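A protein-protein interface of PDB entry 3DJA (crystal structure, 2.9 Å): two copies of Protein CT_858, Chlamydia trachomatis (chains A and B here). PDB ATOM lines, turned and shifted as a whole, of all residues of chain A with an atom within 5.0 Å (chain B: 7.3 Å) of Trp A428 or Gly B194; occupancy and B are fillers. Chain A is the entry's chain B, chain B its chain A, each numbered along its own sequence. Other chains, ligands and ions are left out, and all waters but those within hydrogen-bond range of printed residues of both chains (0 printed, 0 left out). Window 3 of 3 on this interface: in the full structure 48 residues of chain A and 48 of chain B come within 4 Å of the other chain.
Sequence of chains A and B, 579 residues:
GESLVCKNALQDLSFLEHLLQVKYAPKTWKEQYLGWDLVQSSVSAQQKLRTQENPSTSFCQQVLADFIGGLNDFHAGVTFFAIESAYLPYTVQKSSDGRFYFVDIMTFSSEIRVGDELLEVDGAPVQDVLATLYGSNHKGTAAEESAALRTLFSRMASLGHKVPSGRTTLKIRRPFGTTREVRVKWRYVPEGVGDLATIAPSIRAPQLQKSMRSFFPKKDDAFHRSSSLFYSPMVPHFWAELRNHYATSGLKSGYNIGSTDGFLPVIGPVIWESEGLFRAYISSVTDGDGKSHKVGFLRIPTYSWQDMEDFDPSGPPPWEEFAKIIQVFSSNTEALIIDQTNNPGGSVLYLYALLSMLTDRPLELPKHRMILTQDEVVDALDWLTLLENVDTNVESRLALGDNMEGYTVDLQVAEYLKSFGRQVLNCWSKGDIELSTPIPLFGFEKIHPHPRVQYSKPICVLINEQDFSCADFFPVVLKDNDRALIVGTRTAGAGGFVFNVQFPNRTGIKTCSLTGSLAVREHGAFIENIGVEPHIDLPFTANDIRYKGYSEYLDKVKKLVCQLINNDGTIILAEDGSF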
ATOM      1  N   LEU A 372      24.629  25.011  16.304  1.00  0.00           N
ATOM      2  CA  LEU A 372      25.052  24.096  15.261  1.00  0.00           C
ATOM      3  C   LEU A 372      26.534  24.023  14.923  1.00  0.00           C
ATOM      4  O   LEU A 372      27.265  25.025  14.950  1.00  0.00           O
ATOM      5  CB  LEU A 372      24.284  24.415  13.985  1.00  0.00           C
ATOM      6  CG  LEU A 372      22.783  24.542  14.239  1.00  0.00           C
ATOM      7  CD1 LEU A 372      22.055  25.034  13.010  1.00  0.00           C
ATOM      8  CD2 LEU A 372      22.258  23.207  14.657  1.00  0.00           C
ATOM      9  N   THR A 373      26.963  22.804  14.620  1.00  0.00           N
ATOM     10  CA  THR A 373      28.321  22.525  14.171  1.00  0.00           C
ATOM     11  C   THR A 373      28.064  21.616  12.967  1.00  0.00           C
ATOM     12  O   THR A 373      26.933  21.141  12.774  1.00  0.00           O
ATOM     13  CB  THR A 373      29.175  21.783  15.217  1.00  0.00           C
ATOM     14  OG1 THR A 373      28.536  20.560  15.599  1.00  0.00           O
ATOM     15  CG2 THR A 373      29.396  22.659  16.423  1.00  0.00           C
ATOM     16  N   GLN A 374      29.078  21.376  12.148  1.00  0.00           N
ATOM     17  CA  GLN A 374      28.847  20.548  10.990  1.00  0.00           C
ATOM     18  C   GLN A 374      28.302  19.169  11.388  1.00  0.00           C
ATOM     19  O   GLN A 374      27.543  18.566  10.621  1.00  0.00           O
ATOM     20  CB  GLN A 374      30.108  20.466  10.121  1.00  0.00           C
ATOM     21  CG  GLN A 374      31.388  20.898  10.813  1.00  0.00           C
ATOM     22  CD  GLN A 374      31.641  22.409  10.838  1.00  0.00           C
ATOM     23  OE1 GLN A 374      31.737  23.066   9.794  1.00  0.00           O
ATOM     24  NE2 GLN A 374      31.782  22.956  12.043  1.00  0.00           N
ATOM     25  N   VAL A 377      24.724  19.231  11.083  1.00  0.00           N
ATOM     26  CA  VAL A 377      24.414  19.351   9.665  1.00  0.00           C
ATOM     27  C   VAL A 377      24.362  17.978   9.010  1.00  0.00           C
ATOM     28  O   VAL A 377      23.447  17.664   8.259  1.00  0.00           O
ATOM     29  CB  VAL A 377      25.483  20.173   8.912  1.00  0.00           C
ATOM     30  CG1 VAL A 377      25.105  20.264   7.439  1.00  0.00           C
ATOM     31  CG2 VAL A 377      25.618  21.547   9.533  1.00  0.00           C
ATOM     32  N   VAL A 424      17.310  22.264   9.880  1.00  0.00           N
ATOM     33  CA  VAL A 424      18.662  22.396  10.393  1.00  0.00           C
ATOM     34  C   VAL A 424      19.544  22.917   9.280  1.00  0.00           C
ATOM     35  O   VAL A 424      20.287  23.878   9.469  1.00  0.00           O
ATOM     36  CB  VAL A 424      19.213  21.058  10.894  1.00  0.00           C
ATOM     37  CG1 VAL A 424      20.597  21.266  11.528  1.00  0.00           C
ATOM     38  CG2 VAL A 424      18.244  20.462  11.903  1.00  0.00           C
ATOM     39  N   LEU A 425      19.437  22.299   8.109  1.00  0.00           N
ATOM     40  CA  LEU A 425      20.242  22.732   6.979  1.00  0.00           C
ATOM     41  C   LEU A 425      19.980  24.186   6.670  1.00  0.00           C
ATOM     42  O   LEU A 425      20.925  24.930   6.385  1.00  0.00           O
ATOM     43  CB  LEU A 425      19.961  21.897   5.739  1.00  0.00           C
ATOM     44  CG  LEU A 425      20.400  20.442   5.822  1.00  0.00           C
ATOM     45  CD1 LEU A 425      19.998  19.737   4.551  1.00  0.00           C
ATOM     46  CD2 LEU A 425      21.904  20.362   6.039  1.00  0.00           C
ATOM     47  N   ASN A 426      18.719  24.611   6.739  1.00  0.00           N
ATOM     48  CA  ASN A 426      18.421  26.007   6.442  1.00  0.00           C
ATOM     49  C   ASN A 426      19.029  26.988   7.439  1.00  0.00           C
ATOM     50  O   ASN A 426      19.422  28.081   7.060  1.00  0.00           O
ATOM     51  CB  ASN A 426      16.918  26.252   6.340  1.00  0.00           C
ATOM     52  CG  ASN A 426      16.595  27.679   5.887  1.00  0.00           C
ATOM     53  OD1 ASN A 426      17.137  28.153   4.884  1.00  0.00           O
ATOM     54  ND2 ASN A 426      15.719  28.366   6.624  1.00  0.00           N
ATOM     55  N   CYS A 427      19.108  26.619   8.710  1.00  0.00           N
ATOM     56  CA  CYS A 427      19.705  27.532   9.676  1.00  0.00           C
ATOM     57  C   CYS A 427      21.193  27.630   9.412  1.00  0.00           C
ATOM     58  O   CYS A 427      21.812  28.669   9.654  1.00  0.00           O
ATOM     59  CB  CYS A 427      19.492  27.047  11.106  1.00  0.00           C
ATOM     60  SG  CYS A 427      17.788  27.045  11.593  1.00  0.00           S
ATOM     61  N   TRP A 428      21.763  26.538   8.909  1.00  0.00           N
ATOM     62  CA  TRP A 428      23.180  26.488   8.624  1.00  0.00           C
ATOM     63  C   TRP A 428      23.538  27.449   7.505  1.00  0.00           C
ATOM     64  O   TRP A 428      24.397  28.333   7.668  1.00  0.00           O
ATOM     65  CB  TRP A 428      23.586  25.069   8.240  1.00  0.00           C
ATOM     66  CG  TRP A 428      25.055  24.924   8.057  1.00  0.00           C
ATOM     67  CD1 TRP A 428      25.717  24.769   6.876  1.00  0.00           C
ATOM     68  CD2 TRP A 428      26.052  24.969   9.073  1.00  0.00           C
ATOM     69  NE1 TRP A 428      27.066  24.719   7.092  1.00  0.00           N
ATOM     70  CE2 TRP A 428      27.302  24.841   8.440  1.00  0.00           C
ATOM     71  CE3 TRP A 428      26.015  25.107  10.463  1.00  0.00           C
ATOM     72  CZ2 TRP A 428      28.508  24.843   9.147  1.00  0.00           C
ATOM     73  CZ3 TRP A 428      27.210  25.108  11.167  1.00  0.00           C
ATOM     74  CH2 TRP A 428      28.443  24.976  10.503  1.00  0.00           C
ATOM     75  N   SER A 429      22.871  27.284   6.368  1.00  0.00           N
ATOM     76  CA  SER A 429      23.143  28.135   5.218  1.00  0.00           C
ATOM     77  C   SER A 429      22.874  29.596   5.541  1.00  0.00           C
ATOM     78  O   SER A 429      23.561  30.476   5.039  1.00  0.00           O
ATOM     79  CB  SER A 429      22.297  27.707   4.019  1.00  0.00           C
ATOM     80  OG  SER A 429      20.927  27.934   4.277  1.00  0.00           O
ATOM     81  N   LYS A 430      21.889  29.857   6.387  1.00  0.00           N
ATOM     82  CA  LYS A 430      21.574  31.231   6.734  1.00  0.00           C
ATOM     83  C   LYS A 430      22.488  31.799   7.819  1.00  0.00           C
ATOM     84  O   LYS A 430      22.453  33.000   8.101  1.00  0.00           O
ATOM     85  CB  LYS A 430      20.115  31.350   7.165  1.00  0.00           C
ATOM     86  CG  LYS A 430      19.132  31.258   6.015  1.00  0.00           C
ATOM     87  CD  LYS A 430      17.705  31.499   6.474  1.00  0.00           C
ATOM     88  CE  LYS A 430      16.719  31.395   5.308  1.00  0.00           C
ATOM     89  NZ  LYS A 430      15.286  31.543   5.736  1.00  0.00           N
ATOM     90  N   GLY A 431      23.308  30.944   8.424  1.00  0.00           N
ATOM     91  CA  GLY A 431      24.220  31.410   9.454  1.00  0.00           C
ATOM     92  C   GLY A 431      23.626  31.458  10.846  1.00  0.00           C
ATOM     93  O   GLY A 431      24.296  31.847  11.800  1.00  0.00           O
ATOM     94  N   ASP A 432      22.361  31.069  10.960  1.00  0.00           N
ATOM     95  CA  ASP A 432      21.663  31.042  12.234  1.00  0.00           C
ATOM     96  C   ASP A 432      22.224  29.848  12.995  1.00  0.00           C
ATOM     97  O   ASP A 432      21.511  28.874  13.248  1.00  0.00           O
ATOM     98  CB  ASP A 432      20.168  30.862  11.949  1.00  0.00           C
ATOM     99  CG  ASP A 432      19.303  30.867  13.209  1.00  0.00           C
ATOM    100  OD1 ASP A 432      19.779  31.318  14.281  1.00  0.00           O
ATOM    101  OD2 ASP A 432      18.129  30.426  13.105  1.00  0.00           O
ATOM    102  N   ILE A 433      23.497  29.908  13.369  1.00  0.00           N
ATOM    103  CA  ILE A 433      24.086  28.758  14.042  1.00  0.00           C
ATOM    104  C   ILE A 433      24.473  28.927  15.506  1.00  0.00           C
ATOM    105  O   ILE A 433      24.869  27.953  16.154  1.00  0.00           O
ATOM    106  CB  ILE A 433      25.319  28.215  13.255  1.00  0.00           C
ATOM    107  CG1 ILE A 433      26.511  29.140  13.425  1.00  0.00           C
ATOM    108  CG2 ILE A 433      24.994  28.109  11.776  1.00  0.00           C
ATOM    109  CD1 ILE A 433      27.782  28.562  12.831  1.00  0.00           C
ATOM    110  N   THR B  57      36.902  26.310   5.072  1.00  0.00           N
ATOM    111  CA  THR B  57      36.848  25.236   6.035  1.00  0.00           C
ATOM    112  C   THR B  57      37.672  24.056   5.566  1.00  0.00           C
ATOM    113  O   THR B  57      38.564  23.597   6.283  1.00  0.00           O
ATOM    114  CB  THR B  57      35.402  24.771   6.279  1.00  0.00           C
ATOM    115  OG1 THR B  57      34.808  25.617   7.264  1.00  0.00           O
ATOM    116  CG2 THR B  57      35.370  23.324   6.765  1.00  0.00           C
ATOM    117  N   PHE B  81      33.455  15.870   8.840  1.00  0.00           N
ATOM    118  CA  PHE B  81      32.037  15.921   8.515  1.00  0.00           C
ATOM    119  C   PHE B  81      31.912  16.571   7.145  1.00  0.00           C
ATOM    120  O   PHE B  81      31.461  17.714   7.015  1.00  0.00           O
ATOM    121  CB  PHE B  81      31.281  16.751   9.557  1.00  0.00           C
ATOM    122  CG  PHE B  81      31.164  16.077  10.897  1.00  0.00           C
ATOM    123  CD1 PHE B  81      31.526  16.740  12.063  1.00  0.00           C
ATOM    124  CD2 PHE B  81      30.697  14.770  10.992  1.00  0.00           C
ATOM    125  CE1 PHE B  81      31.423  16.104  13.307  1.00  0.00           C
ATOM    126  CE2 PHE B  81      30.592  14.133  12.225  1.00  0.00           C
ATOM    127  CZ  PHE B  81      30.956  14.800  13.382  1.00  0.00           C
ATOM    128  N   GLU B 191      29.900  19.014  -2.226  1.00  0.00           N
ATOM    129  CA  GLU B 191      29.876  19.167  -0.782  1.00  0.00           C
ATOM    130  C   GLU B 191      28.489  19.565  -0.279  1.00  0.00           C
ATOM    131  O   GLU B 191      27.917  20.561  -0.720  1.00  0.00           O
ATOM    132  CB  GLU B 191      30.909  20.200  -0.350  1.00  0.00           C
ATOM    133  CG  GLU B 191      31.108  20.244   1.155  1.00  0.00           C
ATOM    134  CD  GLU B 191      31.290  18.853   1.733  1.00  0.00           C
ATOM    135  OE1 GLU B 191      30.269  18.170   1.985  1.00  0.00           O
ATOM    136  OE2 GLU B 191      32.459  18.438   1.910  1.00  0.00           O
ATOM    137  N   GLY B 192      27.952  18.780   0.650  1.00  0.00           N
ATOM    138  CA  GLY B 192      26.631  19.072   1.175  1.00  0.00           C
ATOM    139  C   GLY B 192      26.662  19.796   2.505  1.00  0.00           C
ATOM    140  O   GLY B 192      25.626  20.172   3.053  1.00  0.00           O
ATOM    141  N   VAL B 193      27.856  19.990   3.036  1.00  0.00           N
ATOM    142  CA  VAL B 193      27.988  20.669   4.307  1.00  0.00           C
ATOM    143  C   VAL B 193      28.694  21.992   4.094  1.00  0.00           C
ATOM    144  O   VAL B 193      29.931  22.056   4.018  1.00  0.00           O
ATOM    145  CB  VAL B 193      28.768  19.816   5.312  1.00  0.00           C
ATOM    146  CG1 VAL B 193      28.998  20.593   6.582  1.00  0.00           C
ATOM    147  CG2 VAL B 193      28.001  18.573   5.603  1.00  0.00           C
ATOM    148  N   GLY B 194      27.880  23.038   4.008  1.00  0.00           N
ATOM    149  CA  GLY B 194      28.369  24.387   3.787  1.00  0.00           C
ATOM    150  C   GLY B 194      29.660  24.803   4.454  1.00  0.00           C
ATOM    151  O   GLY B 194      29.856  24.600   5.657  1.00  0.00           O
ATOM    152  N   ASP B 195      30.555  25.383   3.657  1.00  0.00           N
ATOM    153  CA  ASP B 195      31.817  25.855   4.180  1.00  0.00           C
ATOM    154  C   ASP B 195      31.518  27.025   5.113  1.00  0.00           C
ATOM    155  O   ASP B 195      30.791  27.964   4.764  1.00  0.00           O
ATOM    156  CB  ASP B 195      32.734  26.303   3.056  1.00  0.00           C
ATOM    157  CG  ASP B 195      34.135  26.614   3.549  1.00  0.00           C
ATOM    158  OD1 ASP B 195      34.290  27.617   4.278  1.00  0.00           O
ATOM    159  OD2 ASP B 195      35.072  25.843   3.222  1.00  0.00           O
ATOM    160  N   LEU B 196      32.080  26.952   6.312  1.00  0.00           N
ATOM    161  CA  LEU B 196      31.848  27.976   7.305  1.00  0.00           C
ATOM    162  C   LEU B 196      32.355  29.321   6.822  1.00  0.00           C
ATOM    163  O   LEU B 196      31.706  30.340   7.016  1.00  0.00           O
ATOM    164  CB  LEU B 196      32.523  27.586   8.623  1.00  0.00           C
ATOM    165  CG  LEU B 196      31.723  27.938   9.878  1.00  0.00           C
ATOM    166  CD1 LEU B 196      32.472  27.491  11.105  1.00  0.00           C
ATOM    167  CD2 LEU B 196      31.495  29.426   9.933  1.00  0.00           C
ATOM    168  N   ALA B 197      33.515  29.327   6.187  1.00  0.00           N
ATOM    169  CA  ALA B 197      34.078  30.567   5.693  1.00  0.00           C
ATOM    170  C   ALA B 197      33.076  31.270   4.783  1.00  0.00           C
ATOM    171  O   ALA B 197      33.040  32.502   4.712  1.00  0.00           O
ATOM    172  CB  ALA B 197      35.363  30.292   4.947  1.00  0.00           C
ATOM    173  N   THR B 198      32.256  30.493   4.090  1.00  0.00           N
ATOM    174  CA  THR B 198      31.260  31.078   3.205  1.00  0.00           C
ATOM    175  C   THR B 198      30.087  31.686   3.967  1.00  0.00           C
ATOM    176  O   THR B 198      29.403  32.558   3.453  1.00  0.00           O
ATOM    177  CB  THR B 198      30.687  30.038   2.255  1.00  0.00           C
ATOM    178  OG1 THR B 198      31.718  29.572   1.382  1.00  0.00           O
ATOM    179  CG2 THR B 198      29.561  30.633   1.440  1.00  0.00           C
ATOM    180  N   ILE B 199      29.856  31.225   5.189  1.00  0.00           N
ATOM    181  CA  ILE B 199      28.743  31.718   5.982  1.00  0.00           C
ATOM    182  C   ILE B 199      29.159  32.673   7.088  1.00  0.00           C
ATOM    183  O   ILE B 199      28.350  33.464   7.563  1.00  0.00           O
ATOM    184  CB  ILE B 199      28.006  30.552   6.632  1.00  0.00           C
ATOM    185  CG1 ILE B 199      27.726  29.475   5.591  1.00  0.00           C
ATOM    186  CG2 ILE B 199      26.698  31.036   7.214  1.00  0.00           C
ATOM    187  CD1 ILE B 199      27.087  28.226   6.173  1.00  0.00           C
ATOM    188  N   SER B 202      27.693  36.195   7.631  1.00  0.00           N
ATOM    189  CA  SER B 202      26.275  36.368   7.901  1.00  0.00           C
ATOM    190  C   SER B 202      25.832  35.849   9.272  1.00  0.00           C
ATOM    191  O   SER B 202      24.641  35.847   9.577  1.00  0.00           O
ATOM    192  CB  SER B 202      25.446  35.699   6.806  1.00  0.00           C
ATOM    193  OG  SER B 202      25.300  34.311   7.051  1.00  0.00           O
ATOM    194  N   ILE B 203      26.783  35.416  10.095  1.00  0.00           N
ATOM    195  CA  ILE B 203      26.475  34.897  11.426  1.00  0.00           C
ATOM    196  C   ILE B 203      26.385  36.009  12.444  1.00  0.00           C
ATOM    197  O   ILE B 203      27.413  36.456  12.939  1.00  0.00           O
ATOM    198  CB  ILE B 203      27.579  33.966  11.956  1.00  0.00           C
ATOM    199  CG1 ILE B 203      27.704  32.716  11.093  1.00  0.00           C
ATOM    200  CG2 ILE B 203      27.290  33.608  13.409  1.00  0.00           C
ATOM    201  CD1 ILE B 203      28.942  31.900  11.450  1.00  0.00           C
ATOM    202  N   ASN B 505      33.418  21.007  17.645  1.00  0.00           N
ATOM    203  CA  ASN B 505      34.305  21.986  17.049  1.00  0.00           C
ATOM    204  C   ASN B 505      33.699  22.530  15.771  1.00  0.00           C
ATOM    205  O   ASN B 505      32.811  21.922  15.199  1.00  0.00           O
ATOM    206  CB  ASN B 505      35.639  21.319  16.740  1.00  0.00           C
ATOM    207  CG  ASN B 505      35.541  20.345  15.597  1.00  0.00           C
ATOM    208  OD1 ASN B 505      35.520  20.734  14.424  1.00  0.00           O
ATOM    209  ND2 ASN B 505      35.466  19.063  15.927  1.00  0.00           N
ATOM    210  N   ARG B 506      34.175  23.677  15.312  1.00  0.00           N
ATOM    211  CA  ARG B 506      33.627  24.224  14.092  1.00  0.00           C
ATOM    212  C   ARG B 506      34.515  24.042  12.881  1.00  0.00           C
ATOM    213  O   ARG B 506      34.301  24.672  11.848  1.00  0.00           O
ATOM    214  CB  ARG B 506      33.256  25.691  14.287  1.00  0.00           C
ATOM    215  CG  ARG B 506      31.836  25.807  14.794  1.00  0.00           C
ATOM    216  CD  ARG B 506      31.520  27.138  15.427  1.00  0.00           C
ATOM    217  NE  ARG B 506      30.153  27.128  15.946  1.00  0.00           N
ATOM    218  CZ  ARG B 506      29.663  28.042  16.773  1.00  0.00           C
ATOM    219  NH1 ARG B 506      30.429  29.051  17.185  1.00  0.00           N
ATOM    220  NH2 ARG B 506      28.410  27.941  17.191  1.00  0.00           N
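O of Lys A430 is in hydrogen-bond range of OG of Ser B202, at 3.3 Å.
NE2 of Gln A374 sits close to O of Arg B506, 3.1 Å away.
The side-chain amide nitrogen of Gln A374 is in hydrogen-bond range of the backbone carbonyl oxygen of Asn B505, 3.5 Å away.
O of Gly B194 sits at hydrogen-bond distance from NE1 of Trp A428 (3.1 Å).
The side-chain hydroxyl of Ser B202 is in hydrogen-bond range of the backbone carbonyl oxygen of Ile B199 (3.2 Å).
O of Asn A426 lies within hydrogen-bond range of OG of Ser A429, 3.2 Å away.
ND2 of Asn A426 sits close to NZ of Lys A430 (3.3 Å).
The side-chain carboxylate (OE1) of Glu B191 sits at hydrogen-bond distance from the backbone NH (N) of Val B193, 3.2 Å away.
The backbone NH of Leu A372 lies within hydrogen-bond range of the backbone carbonyl oxygen of Ile A433.
Leu A372 touches Arg B506.
Asn B505 touches Thr A373 (O to CB, 3.6 Å).
Val B193 touches Gln A374 (CG1 to CB, 3.7 Å).
CG1 of Val A377 touches CG2 of Val B193 (3.8 Å).
Ile B199 touches Trp A428.
Gly A431 touches Ile B199 (CA to CG2, 3.4 Å).
CA of Gly A431 touches OG of Ser B202, at 3.9 Å.
Gly A431 touches Ile B203.
CD1 of Ile B203 touches CD1 of Ile A433, 3.8 Å away.
Ile A433 touches Arg B506.
Printed residues of chain B within 4 Å of Thr A373: Asn B505 (3.6 Å).
Of chain B, only Gly B194 (3.1 Å) and Ile B199 (3.1 Å) come within 4 Å of Trp A428.
Of the printed residues of chain B, Lys A430 touches Ser B202.
Glu B191 touches none of the printed residues of chain A.
Of the printed residues of chain A, Gly B194 touches Trp A428 (3.1 Å).
Of the printed residues of chain A, Ile B199 touches Trp A428 (3.1 Å), Ser A429 (3.9 Å) and Gly A431 (3.4 Å).
Printed residues of chain A within 4 Å of Asn B505: Thr A373 (3.6 Å) and Gln A374 (3.5 Å).
The nearest residue of chain B that does not touch Trp A428 is Val B193 (4.4 Å).
The nearest printed residue of chain B that does not touch Gln A374 is Leu B196 (4.7 Å).
Of the 14 printed residues of chain A, 9 touch a printed residue of chain B.
Hydrophobic or aromatic side chains of chain A within 4 Å of the printed part of chain B: Val A377, Trp A428 and Ile A433.
Of the 15 printed residues of chain B, 8 touch a printed residue of chain A.
Printed residues of chain B that touch a printed residue of chain A: Phe B81, Val B193, Gly B194, Ile B199, Ser B202, Ile B203, Asn B505 and Arg B506.
Hydrophobic or aromatic side chains of chain B within 4 Å of the printed part of chain A: Phe B81, Val B193, Ile B199 and Ile B203.
Among the printed residues, 16 pairs touch across the chains.
Among the printed residues, no Asp or Glu carboxylate lies within 4 Å of a Lys or Arg side-chain nitrogen of the other chain.
No position is printed for both chains.
Of the 16 pairs that touch across the chains among the printed residues, none has its exchanged pair printed and touching as well.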
